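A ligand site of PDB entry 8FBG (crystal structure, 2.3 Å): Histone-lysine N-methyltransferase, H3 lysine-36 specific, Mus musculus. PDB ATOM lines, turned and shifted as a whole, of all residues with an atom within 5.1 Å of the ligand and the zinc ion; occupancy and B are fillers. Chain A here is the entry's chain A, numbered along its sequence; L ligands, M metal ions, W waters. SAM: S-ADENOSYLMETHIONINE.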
ATOM      1  N   ARG A 102       0.266  18.435  26.625  1.00  0.00           N
ATOM      2  CA  ARG A 102      -0.611  18.044  25.505  1.00  0.00           C
ATOM      3  C   ARG A 102      -0.390  16.587  25.052  1.00  0.00           C
ATOM      4  O   ARG A 102      -0.667  16.247  23.907  1.00  0.00           O
ATOM      5  CB  ARG A 102      -0.434  19.005  24.313  1.00  0.00           C
ATOM      6  CG  ARG A 102      -0.812  20.454  24.604  1.00  0.00           C
ATOM      7  CD  ARG A 102      -0.089  21.406  23.685  1.00  0.00           C
ATOM      8  NE  ARG A 102       1.349  21.323  23.905  1.00  0.00           N
ATOM      9  CZ  ARG A 102       2.247  21.110  22.965  1.00  0.00           C
ATOM     10  NH1 ARG A 102       1.877  21.026  21.687  1.00  0.00           N
ATOM     11  NH2 ARG A 102       3.527  21.007  23.283  1.00  0.00           N
ATOM     12  N   GLY A 103       0.035  15.738  25.982  1.00  0.00           N
ATOM     13  CA  GLY A 103       0.273  14.313  25.756  1.00  0.00           C
ATOM     14  C   GLY A 103       1.438  14.055  24.824  1.00  0.00           C
ATOM     15  O   GLY A 103       2.525  14.622  24.993  1.00  0.00           O
ATOM     16  N   TRP A 104       1.191  13.186  23.830  1.00  0.00           N
ATOM     17  CA  TRP A 104       2.159  12.808  22.800  1.00  0.00           C
ATOM     18  C   TRP A 104       2.082  13.801  21.663  1.00  0.00           C
ATOM     19  O   TRP A 104       0.990  14.230  21.293  1.00  0.00           O
ATOM     20  CB  TRP A 104       1.860  11.394  22.264  1.00  0.00           C
ATOM     21  CG  TRP A 104       2.148  10.333  23.271  1.00  0.00           C
ATOM     22  CD1 TRP A 104       1.261   9.740  24.113  1.00  0.00           C
ATOM     23  CD2 TRP A 104       3.450   9.857  23.661  1.00  0.00           C
ATOM     24  NE1 TRP A 104       1.908   8.851  24.936  1.00  0.00           N
ATOM     25  CE2 TRP A 104       3.255   8.913  24.693  1.00  0.00           C
ATOM     26  CE3 TRP A 104       4.754  10.081  23.188  1.00  0.00           C
ATOM     27  CZ2 TRP A 104       4.325   8.219  25.280  1.00  0.00           C
ATOM     28  CZ3 TRP A 104       5.809   9.391  23.758  1.00  0.00           C
ATOM     29  CH2 TRP A 104       5.596   8.478  24.796  1.00  0.00           C
ATOM     30  N   GLY A 105       3.232  14.157  21.116  1.00  0.00           N
ATOM     31  CA  GLY A 105       3.342  15.073  19.975  1.00  0.00           C
ATOM     32  C   GLY A 105       4.249  14.549  18.885  1.00  0.00           C
ATOM     33  O   GLY A 105       4.868  13.487  19.049  1.00  0.00           O
ATOM     34  N   THR A 144     -10.374  11.578  26.145  1.00  0.00           N
ATOM     35  CA  THR A 144     -10.147  13.019  25.892  1.00  0.00           C
ATOM     36  C   THR A 144      -9.338  13.295  24.602  1.00  0.00           C
ATOM     37  O   THR A 144      -9.267  14.454  24.172  1.00  0.00           O
ATOM     38  CB  THR A 144      -9.472  13.730  27.110  1.00  0.00           C
ATOM     39  OG1 THR A 144      -8.255  13.069  27.463  1.00  0.00           O
ATOM     40  CG2 THR A 144     -10.401  13.802  28.342  1.00  0.00           C
ATOM     41  N   ASN A 145      -8.759  12.214  23.991  1.00  0.00           N
ATOM     42  CA  ASN A 145      -8.000  12.268  22.743  1.00  0.00           C
ATOM     43  C   ASN A 145      -8.856  11.916  21.534  1.00  0.00           C
ATOM     44  O   ASN A 145      -9.458  10.841  21.467  1.00  0.00           O
ATOM     45  CB  ASN A 145      -6.761  11.379  22.792  1.00  0.00           C
ATOM     46  CG  ASN A 145      -5.657  11.942  23.623  1.00  0.00           C
ATOM     47  OD1 ASN A 145      -5.143  13.023  23.360  1.00  0.00           O
ATOM     48  ND2 ASN A 145      -5.256  11.225  24.627  1.00  0.00           N
ATOM     49  N   PHE A 146      -8.887  12.822  20.556  1.00  0.00           N
ATOM     50  CA  PHE A 146      -9.655  12.645  19.342  1.00  0.00           C
ATOM     51  C   PHE A 146      -8.755  12.774  18.134  1.00  0.00           C
ATOM     52  O   PHE A 146      -7.769  13.531  18.158  1.00  0.00           O
ATOM     53  CB  PHE A 146     -10.824  13.626  19.266  1.00  0.00           C
ATOM     54  CG  PHE A 146     -11.846  13.418  20.347  1.00  0.00           C
ATOM     55  CD1 PHE A 146     -12.841  12.452  20.210  1.00  0.00           C
ATOM     56  CD2 PHE A 146     -11.822  14.189  21.514  1.00  0.00           C
ATOM     57  CE1 PHE A 146     -13.782  12.252  21.214  1.00  0.00           C
ATOM     58  CE2 PHE A 146     -12.784  13.984  22.510  1.00  0.00           C
ATOM     59  CZ  PHE A 146     -13.742  13.007  22.357  1.00  0.00           C
ATOM     60  N   TYR A 147      -9.084  12.025  17.074  1.00  0.00           N
ATOM     61  CA  TYR A 147      -8.292  11.973  15.849  1.00  0.00           C
ATOM     62  C   TYR A 147      -9.212  12.155  14.632  1.00  0.00           C
ATOM     63  O   TYR A 147      -8.900  11.678  13.541  1.00  0.00           O
ATOM     64  CB  TYR A 147      -7.460  10.653  15.795  1.00  0.00           C
ATOM     65  CG  TYR A 147      -6.648  10.399  17.054  1.00  0.00           C
ATOM     66  CD1 TYR A 147      -7.225   9.807  18.172  1.00  0.00           C
ATOM     67  CD2 TYR A 147      -5.316  10.765  17.125  1.00  0.00           C
ATOM     68  CE1 TYR A 147      -6.504   9.636  19.344  1.00  0.00           C
ATOM     69  CE2 TYR A 147      -4.578  10.572  18.289  1.00  0.00           C
ATOM     70  CZ  TYR A 147      -5.181  10.027  19.400  1.00  0.00           C
ATOM     71  OH  TYR A 147      -4.464   9.894  20.561  1.00  0.00           O
ATOM     72  N   ARG A 167      -1.470  11.756  13.093  1.00  0.00           N
ATOM     73  CA  ARG A 167      -2.367  11.564  14.223  1.00  0.00           C
ATOM     74  C   ARG A 167      -1.738  12.064  15.561  1.00  0.00           C
ATOM     75  O   ARG A 167      -2.488  12.301  16.497  1.00  0.00           O
ATOM     76  CB  ARG A 167      -2.762  10.085  14.321  1.00  0.00           C
ATOM     77  CG  ARG A 167      -1.767   9.222  15.080  1.00  0.00           C
ATOM     78  CD  ARG A 167      -2.075   7.725  15.007  1.00  0.00           C
ATOM     79  NE  ARG A 167      -3.163   7.278  15.883  1.00  0.00           N
ATOM     80  CZ  ARG A 167      -3.092   7.211  17.211  1.00  0.00           C
ATOM     81  NH1 ARG A 167      -4.120   6.730  17.903  1.00  0.00           N
ATOM     82  NH2 ARG A 167      -2.024   7.646  17.855  1.00  0.00           N
ATOM     83  N   PHE A 168      -0.385  12.221  15.659  1.00  0.00           N
ATOM     84  CA  PHE A 168       0.307  12.713  16.871  1.00  0.00           C
ATOM     85  C   PHE A 168       0.508  14.240  16.864  1.00  0.00           C
ATOM     86  O   PHE A 168       0.865  14.813  17.879  1.00  0.00           O
ATOM     87  CB  PHE A 168       1.648  12.010  17.068  1.00  0.00           C
ATOM     88  CG  PHE A 168       1.470  10.550  17.425  1.00  0.00           C
ATOM     89  CD1 PHE A 168       1.105  10.172  18.720  1.00  0.00           C
ATOM     90  CD2 PHE A 168       1.611   9.558  16.453  1.00  0.00           C
ATOM     91  CE1 PHE A 168       0.894   8.833  19.035  1.00  0.00           C
ATOM     92  CE2 PHE A 168       1.413   8.223  16.783  1.00  0.00           C
ATOM     93  CZ  PHE A 168       1.068   7.875  18.064  1.00  0.00           C
ATOM     94  N   MET A 169       0.211  14.894  15.745  1.00  0.00           N
ATOM     95  CA  MET A 169       0.355  16.329  15.612  1.00  0.00           C
ATOM     96  C   MET A 169      -0.710  17.095  16.422  1.00  0.00           C
ATOM     97  O   MET A 169      -1.917  16.937  16.231  1.00  0.00           O
ATOM     98  CB  MET A 169       0.333  16.727  14.147  1.00  0.00           C
ATOM     99  CG  MET A 169       1.679  16.534  13.503  1.00  0.00           C
ATOM    100  SD  MET A 169       1.775  17.051  11.786  1.00  0.00           S
ATOM    101  CE  MET A 169       1.309  18.775  11.932  1.00  0.00           C
ATOM    102  N   ASN A 170      -0.220  17.911  17.366  1.00  0.00           N
ATOM    103  CA  ASN A 170      -1.049  18.695  18.274  1.00  0.00           C
ATOM    104  C   ASN A 170      -1.495  20.021  17.684  1.00  0.00           C
ATOM    105  O   ASN A 170      -0.925  20.503  16.698  1.00  0.00           O
ATOM    106  CB  ASN A 170      -0.320  18.937  19.586  1.00  0.00           C
ATOM    107  CG  ASN A 170      -0.152  17.722  20.450  1.00  0.00           C
ATOM    108  OD1 ASN A 170      -1.085  16.969  20.686  1.00  0.00           O
ATOM    109  ND2 ASN A 170       1.061  17.508  20.955  1.00  0.00           N
ATOM    110  N   HIS A 171      -2.560  20.594  18.282  1.00  0.00           N
ATOM    111  CA  HIS A 171      -3.082  21.890  17.915  1.00  0.00           C
ATOM    112  C   HIS A 171      -2.163  23.009  18.520  1.00  0.00           C
ATOM    113  O   HIS A 171      -1.625  22.847  19.603  1.00  0.00           O
ATOM    114  CB  HIS A 171      -4.531  22.074  18.445  1.00  0.00           C
ATOM    115  CG  HIS A 171      -4.988  23.478  18.332  1.00  0.00           C
ATOM    116  ND1 HIS A 171      -5.293  24.037  17.098  1.00  0.00           N
ATOM    117  CD2 HIS A 171      -5.014  24.462  19.270  1.00  0.00           C
ATOM    118  CE1 HIS A 171      -5.537  25.310  17.343  1.00  0.00           C
ATOM    119  NE2 HIS A 171      -5.361  25.615  18.622  1.00  0.00           N
ATOM    120  N   CYS A 172      -2.109  24.147  17.829  1.00  0.00           N
ATOM    121  CA  CYS A 172      -1.421  25.358  18.247  1.00  0.00           C
ATOM    122  C   CYS A 172      -2.095  26.577  17.612  1.00  0.00           C
ATOM    123  O   CYS A 172      -2.466  26.531  16.433  1.00  0.00           O
ATOM    124  CB  CYS A 172       0.058  25.297  17.885  1.00  0.00           C
ATOM    125  SG  CYS A 172       1.043  26.632  18.575  1.00  0.00           S
ATOM    126  N   CYS A 173      -2.232  27.653  18.393  1.00  0.00           N
ATOM    127  CA  CYS A 173      -2.780  28.946  17.981  1.00  0.00           C
ATOM    128  C   CYS A 173      -1.756  29.717  17.131  1.00  0.00           C
ATOM    129  O   CYS A 173      -2.128  30.655  16.429  1.00  0.00           O
ATOM    130  CB  CYS A 173      -3.225  29.755  19.187  1.00  0.00           C
ATOM    131  SG  CYS A 173      -4.574  28.997  20.123  1.00  0.00           S
ATOM    132  N   TYR A 208      -6.252  23.419  14.457  1.00  0.00           N
ATOM    133  CA  TYR A 208      -7.361  22.492  14.200  1.00  0.00           C
ATOM    134  C   TYR A 208      -8.549  23.236  13.606  1.00  0.00           C
ATOM    135  O   TYR A 208      -9.319  22.650  12.840  1.00  0.00           O
ATOM    136  CB  TYR A 208      -7.773  21.757  15.499  1.00  0.00           C
ATOM    137  CG  TYR A 208      -6.820  20.696  16.044  1.00  0.00           C
ATOM    138  CD1 TYR A 208      -5.590  20.451  15.443  1.00  0.00           C
ATOM    139  CD2 TYR A 208      -7.172  19.927  17.159  1.00  0.00           C
ATOM    140  CE1 TYR A 208      -4.741  19.456  15.920  1.00  0.00           C
ATOM    141  CE2 TYR A 208      -6.317  18.937  17.656  1.00  0.00           C
ATOM    142  CZ  TYR A 208      -5.096  18.709  17.043  1.00  0.00           C
ATOM    143  OH  TYR A 208      -4.246  17.765  17.557  1.00  0.00           O
ATOM    144  N   ASN A 215     -13.443  17.930  20.573  1.00  0.00           N
ATOM    145  CA  ASN A 215     -12.683  18.734  21.567  1.00  0.00           C
ATOM    146  C   ASN A 215     -13.492  19.924  22.126  1.00  0.00           C
ATOM    147  O   ASN A 215     -13.096  21.076  21.976  1.00  0.00           O
ATOM    148  CB  ASN A 215     -11.353  19.225  20.958  1.00  0.00           C
ATOM    149  CG  ASN A 215     -10.483  18.121  20.424  1.00  0.00           C
ATOM    150  OD1 ASN A 215     -10.179  17.156  21.128  1.00  0.00           O
ATOM    151  ND2 ASN A 215     -10.050  18.236  19.175  1.00  0.00           N
ATOM    152  N   THR A 218     -12.065  21.173  26.067  1.00  0.00           N
ATOM    153  CA  THR A 218     -10.617  20.986  26.132  1.00  0.00           C
ATOM    154  C   THR A 218      -9.914  22.368  26.219  1.00  0.00           C
ATOM    155  O   THR A 218     -10.138  23.240  25.376  1.00  0.00           O
ATOM    156  CB  THR A 218     -10.125  20.117  24.959  1.00  0.00           C
ATOM    157  OG1 THR A 218     -10.899  18.907  24.917  1.00  0.00           O
ATOM    158  CG2 THR A 218      -8.621  19.787  25.052  1.00  0.00           C
ATOM    159  N   VAL A 219      -9.105  22.555  27.264  1.00  0.00           N
ATOM    160  CA  VAL A 219      -8.356  23.802  27.485  1.00  0.00           C
ATOM    161  C   VAL A 219      -7.060  23.765  26.634  1.00  0.00           C
ATOM    162  O   VAL A 219      -6.281  22.814  26.765  1.00  0.00           O
ATOM    163  CB  VAL A 219      -8.091  24.049  29.014  1.00  0.00           C
ATOM    164  CG1 VAL A 219      -7.056  25.143  29.266  1.00  0.00           C
ATOM    165  CG2 VAL A 219      -9.389  24.357  29.755  1.00  0.00           C
ATOM    166  N   CYS A 220      -6.863  24.770  25.748  1.00  0.00           N
ATOM    167  CA  CYS A 220      -5.668  24.806  24.893  1.00  0.00           C
ATOM    168  C   CYS A 220      -4.423  25.055  25.708  1.00  0.00           C
ATOM    169  O   CYS A 220      -4.335  26.057  26.406  1.00  0.00           O
ATOM    170  CB  CYS A 220      -5.799  25.832  23.780  1.00  0.00           C
ATOM    171  SG  CYS A 220      -4.396  25.829  22.634  1.00  0.00           S
ATOM    172  N   LYS A 221      -3.446  24.146  25.583  1.00  0.00           N
ATOM    173  CA  LYS A 221      -2.180  24.234  26.296  1.00  0.00           C
ATOM    174  C   LYS A 221      -1.009  24.474  25.319  1.00  0.00           C
ATOM    175  O   LYS A 221       0.116  24.139  25.681  1.00  0.00           O
ATOM    176  CB  LYS A 221      -1.942  22.959  27.145  1.00  0.00           C
ATOM    177  CG  LYS A 221      -3.003  22.654  28.227  1.00  0.00           C
ATOM    178  CD  LYS A 221      -2.827  23.497  29.495  1.00  0.00           C
ATOM    179  CE  LYS A 221      -3.621  22.984  30.673  1.00  0.00           C
ATOM    180  NZ  LYS A 221      -3.236  23.662  31.947  1.00  0.00           N
ATOM    181  N   CYS A 222      -1.255  25.074  24.100  1.00  0.00           N
ATOM    182  CA  CYS A 222      -0.187  25.345  23.122  1.00  0.00           C
ATOM    183  C   CYS A 222       0.877  26.321  23.687  1.00  0.00           C
ATOM    184  O   CYS A 222       2.040  26.229  23.289  1.00  0.00           O
ATOM    185  CB  CYS A 222      -0.728  25.828  21.769  1.00  0.00           C
ATOM    186  SG  CYS A 222      -1.252  27.573  21.707  1.00  0.00           S
ATOM    187  N   GLY A 223       0.477  27.212  24.610  1.00  0.00           N
ATOM    188  CA  GLY A 223       1.363  28.148  25.283  1.00  0.00           C
ATOM    189  C   GLY A 223       1.895  29.275  24.422  1.00  0.00           C
ATOM    190  O   GLY A 223       2.917  29.857  24.744  1.00  0.00           O
ATOM    191  N   CYS A 227      -2.608  32.781  22.261  1.00  0.00           N
ATOM    192  CA  CYS A 227      -3.524  31.669  22.513  1.00  0.00           C
ATOM    193  C   CYS A 227      -4.955  32.148  22.862  1.00  0.00           C
ATOM    194  O   CYS A 227      -5.103  32.970  23.747  1.00  0.00           O
ATOM    195  CB  CYS A 227      -2.984  30.749  23.602  1.00  0.00           C
ATOM    196  SG  CYS A 227      -3.996  29.261  23.883  1.00  0.00           S
ATOM    197  N   SER A 228      -5.972  31.580  22.207  1.00  0.00           N
ATOM    198  CA  SER A 228      -7.388  31.895  22.447  1.00  0.00           C
ATOM    199  C   SER A 228      -7.998  31.053  23.615  1.00  0.00           C
ATOM    200  O   SER A 228      -9.092  31.351  24.057  1.00  0.00           O
ATOM    201  CB  SER A 228      -8.213  31.736  21.166  1.00  0.00           C
ATOM    202  OG  SER A 228      -8.352  30.387  20.740  1.00  0.00           O
ATOM    203  N   GLY A 229      -7.270  30.060  24.105  1.00  0.00           N
ATOM    204  CA  GLY A 229      -7.671  29.214  25.222  1.00  0.00           C
ATOM    205  C   GLY A 229      -8.403  27.935  24.842  1.00  0.00           C
ATOM    206  O   GLY A 229      -8.544  27.024  25.671  1.00  0.00           O
ATOM    207  N   PHE A 230      -8.853  27.858  23.578  1.00  0.00           N
ATOM    208  CA  PHE A 230      -9.625  26.749  23.032  1.00  0.00           C
ATOM    209  C   PHE A 230      -8.921  26.103  21.836  1.00  0.00           C
ATOM    210  O   PHE A 230      -8.185  26.792  21.128  1.00  0.00           O
ATOM    211  CB  PHE A 230     -11.027  27.231  22.620  1.00  0.00           C
ATOM    212  CG  PHE A 230     -11.670  28.185  23.591  1.00  0.00           C
ATOM    213  N   LEU A 231      -9.165  24.792  21.621  1.00  0.00           N
ATOM    214  CA  LEU A 231      -8.616  24.036  20.496  1.00  0.00           C
ATOM    215  C   LEU A 231      -9.345  24.452  19.228  1.00  0.00           C
ATOM    216  O   LEU A 231     -10.569  24.344  19.147  1.00  0.00           O
ATOM    217  CB  LEU A 231      -8.765  22.498  20.671  1.00  0.00           C
ATOM    218  CG  LEU A 231      -8.020  21.783  21.792  1.00  0.00           C
ATOM    219  CD1 LEU A 231      -7.740  20.359  21.399  1.00  0.00           C
ATOM    220  CD2 LEU A 231      -6.738  22.464  22.119  1.00  0.00           C
HETATM  221  N   SAM L   1      -1.729  14.553  21.936  1.00  0.00           N
HETATM  222  CA  SAM L   1      -2.338  13.459  21.162  1.00  0.00           C
HETATM  223  C   SAM L   1      -1.856  12.073  21.712  1.00  0.00           C
HETATM  224  O   SAM L   1      -1.271  12.139  22.811  1.00  0.00           O
HETATM  225  OXT SAM L   1      -2.127  11.023  21.088  1.00  0.00           O
HETATM  226  CB  SAM L   1      -1.981  13.580  19.657  1.00  0.00           C
HETATM  227  CG  SAM L   1      -2.839  14.676  18.940  1.00  0.00           C
HETATM  228  SD  SAM L   1      -4.499  14.077  18.778  1.00  0.00           S
HETATM  229  CE  SAM L   1      -4.811  14.396  17.087  1.00  0.00           C
HETATM  230  C5' SAM L   1      -5.383  15.449  19.496  1.00  0.00           C
HETATM  231  C4' SAM L   1      -5.725  15.326  20.988  1.00  0.00           C
HETATM  232  O4' SAM L   1      -4.586  15.791  21.753  1.00  0.00           O
HETATM  233  C3' SAM L   1      -6.902  16.213  21.406  1.00  0.00           C
HETATM  234  O3' SAM L   1      -8.119  15.476  21.421  1.00  0.00           O
HETATM  235  C2' SAM L   1      -6.500  16.689  22.809  1.00  0.00           C
HETATM  236  O2' SAM L   1      -6.888  15.761  23.817  1.00  0.00           O
HETATM  237  C1' SAM L   1      -4.973  16.761  22.693  1.00  0.00           C
HETATM  238  N9  SAM L   1      -4.442  18.066  22.290  1.00  0.00           N
HETATM  239  C8  SAM L   1      -3.947  18.397  21.046  1.00  0.00           C
HETATM  240  N7  SAM L   1      -3.548  19.636  20.946  1.00  0.00           N
HETATM  241  C5  SAM L   1      -3.794  20.168  22.210  1.00  0.00           C
HETATM  242  C6  SAM L   1      -3.675  21.476  22.725  1.00  0.00           C
HETATM  243  N6  SAM L   1      -3.238  22.511  22.015  1.00  0.00           N
HETATM  244  N1  SAM L   1      -4.072  21.686  24.007  1.00  0.00           N
HETATM  245  C2  SAM L   1      -4.544  20.646  24.710  1.00  0.00           C
HETATM  246  N3  SAM L   1      -4.693  19.374  24.337  1.00  0.00           N
HETATM  247  C4  SAM L   1      -4.321  19.202  23.050  1.00  0.00           C
HETATM  248 ZN    ZN M   1      -3.517  27.865  22.080  1.00  0.00          ZN
HETATM  249  O   HOH W   1      -2.538  11.186  25.323  1.00  0.00           O
HETATM  250  O   HOH W   2      -1.545   8.552  22.052  1.00  0.00           O
HETATM  251  O   HOH W   3      -3.157  14.623  24.324  1.00  0.00           O
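Water W3 lies within hydrogen-bond range of OD1 of Asn 145, N of the ligand and O of Arg 102. Water W1 bridges the side-chain amide nitrogen (ND2) of Asn 145 and an oxygen (O) of the ligand.
The backbone carbonyl oxygen of Arg 102 lies within hydrogen-bond range of a nitrogen (N) of the ligand, 2.8 Å away. The backbone carbonyl oxygen of Trp 104 is in hydrogen-bond range of a nitrogen (N) of the ligand. OD1 of Asn 145 sits close to O4' of the ligand, 3.2 Å away. A nitrogen (N1) of the ligand sits at hydrogen-bond distance from the backbone NH (N) of Lys 221. The side-chain amide oxygen (OD1) of Asn 170 sits at hydrogen-bond distance from a nitrogen (N) of the ligand. The backbone NH (N) of His 171 is in hydrogen-bond range of a nitrogen (N7) of the ligand (3.0 Å). The side-chain amide oxygen (OD1) of Asn 215 sits at hydrogen-bond distance from an oxygen (O3') of the ligand (2.7 Å). The backbone carbonyl oxygen (O) of Thr 144 lies within hydrogen-bond range of an oxygen (O2') of the ligand, 2.7 Å away. The backbone NH (N) of Trp 104 is in hydrogen-bond range of an oxygen (O) of the ligand. The backbone NH (N) of Phe 146 is in hydrogen-bond range of an oxygen (O3') of the ligand. The side-chain sulfur (SG) of Cys 220 lies close to a nitrogen (N6) of the ligand (3.6 Å). The backbone carbonyl oxygen of His 171 is in hydrogen-bond range of a nitrogen (N6) of the ligand, at 2.9 Å. OXT of the ligand sits at hydrogen-bond distance from OH of Tyr 147 (2.6 Å).
The backbone carbonyl oxygen (O) of Arg 167 lies close to a sulfur (SD) of the ligand. Gly 103 touches the ligand. Phe 168 touches the ligand (O to CB, 3.6 Å). Met 169 touches the ligand (O to CG, 3.6 Å). OH of Tyr 208 touches C5' of the ligand, 3.2 Å away. Val 219 touches the ligand (O to C2, 3.5 Å). Leu 231 touches the ligand (CD2 to C6, 3.3 Å). 19 residues have an atom within 4 Å of the ligand: Arg 102, Gly 103, Trp 104, Thr 144, Asn 145, Phe 146, Tyr 147, Arg 167, Phe 168, Met 169, Asn 170, His 171, Tyr 208, Asn 215, Val 219, Cys 220, Lys 221, Cys 222 and Leu 231. Along chain A the residues within 4 Å of the ligand span positions 102 to 231.
A ring nitrogen (ND1) of His 171 lies within hydrogen-bond range of the backbone NH (N) of Tyr 208 (2.9 Å). The backbone carbonyl oxygen (O) of Trp 104 sits at hydrogen-bond distance from the side-chain amide nitrogen (ND2) of Asn 170 (3.3 Å). OD1 of Asn 170 lies close to O of Arg 102 (3.3 Å). SG of Cys 173 sits close to N of Ser 228 (3.6 Å). The backbone NH of Cys 220 is in hydrogen-bond range of the backbone carbonyl oxygen of Gly 229 (2.8 Å). The backbone NH (N) of Gly 229 lies close to the side-chain sulfur (SG) of Cys 227, 3.4 Å away. OH of Tyr 208 sits at hydrogen-bond distance from O of Met 169 (2.8 Å). NE2 of His 171 lies close to SG of Cys 173.
The zinc ion is bound by SG of Cys 220 (2.3 Å), SG of Cys 222 (2.3 Å), SG of Cys 227 (2.3 Å) and SG of Cys 173 (2.5 Å). The zinc ion has four donor atoms within binding distance.
Of the 28 residues printed, 4 come within 4 Å of the zinc ion. Along chain A the residues within 4 Å of the zinc ion span positions 173 to 227. The nearest printed residue that does not touch the zinc ion is Ser 228 (4.5 Å).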
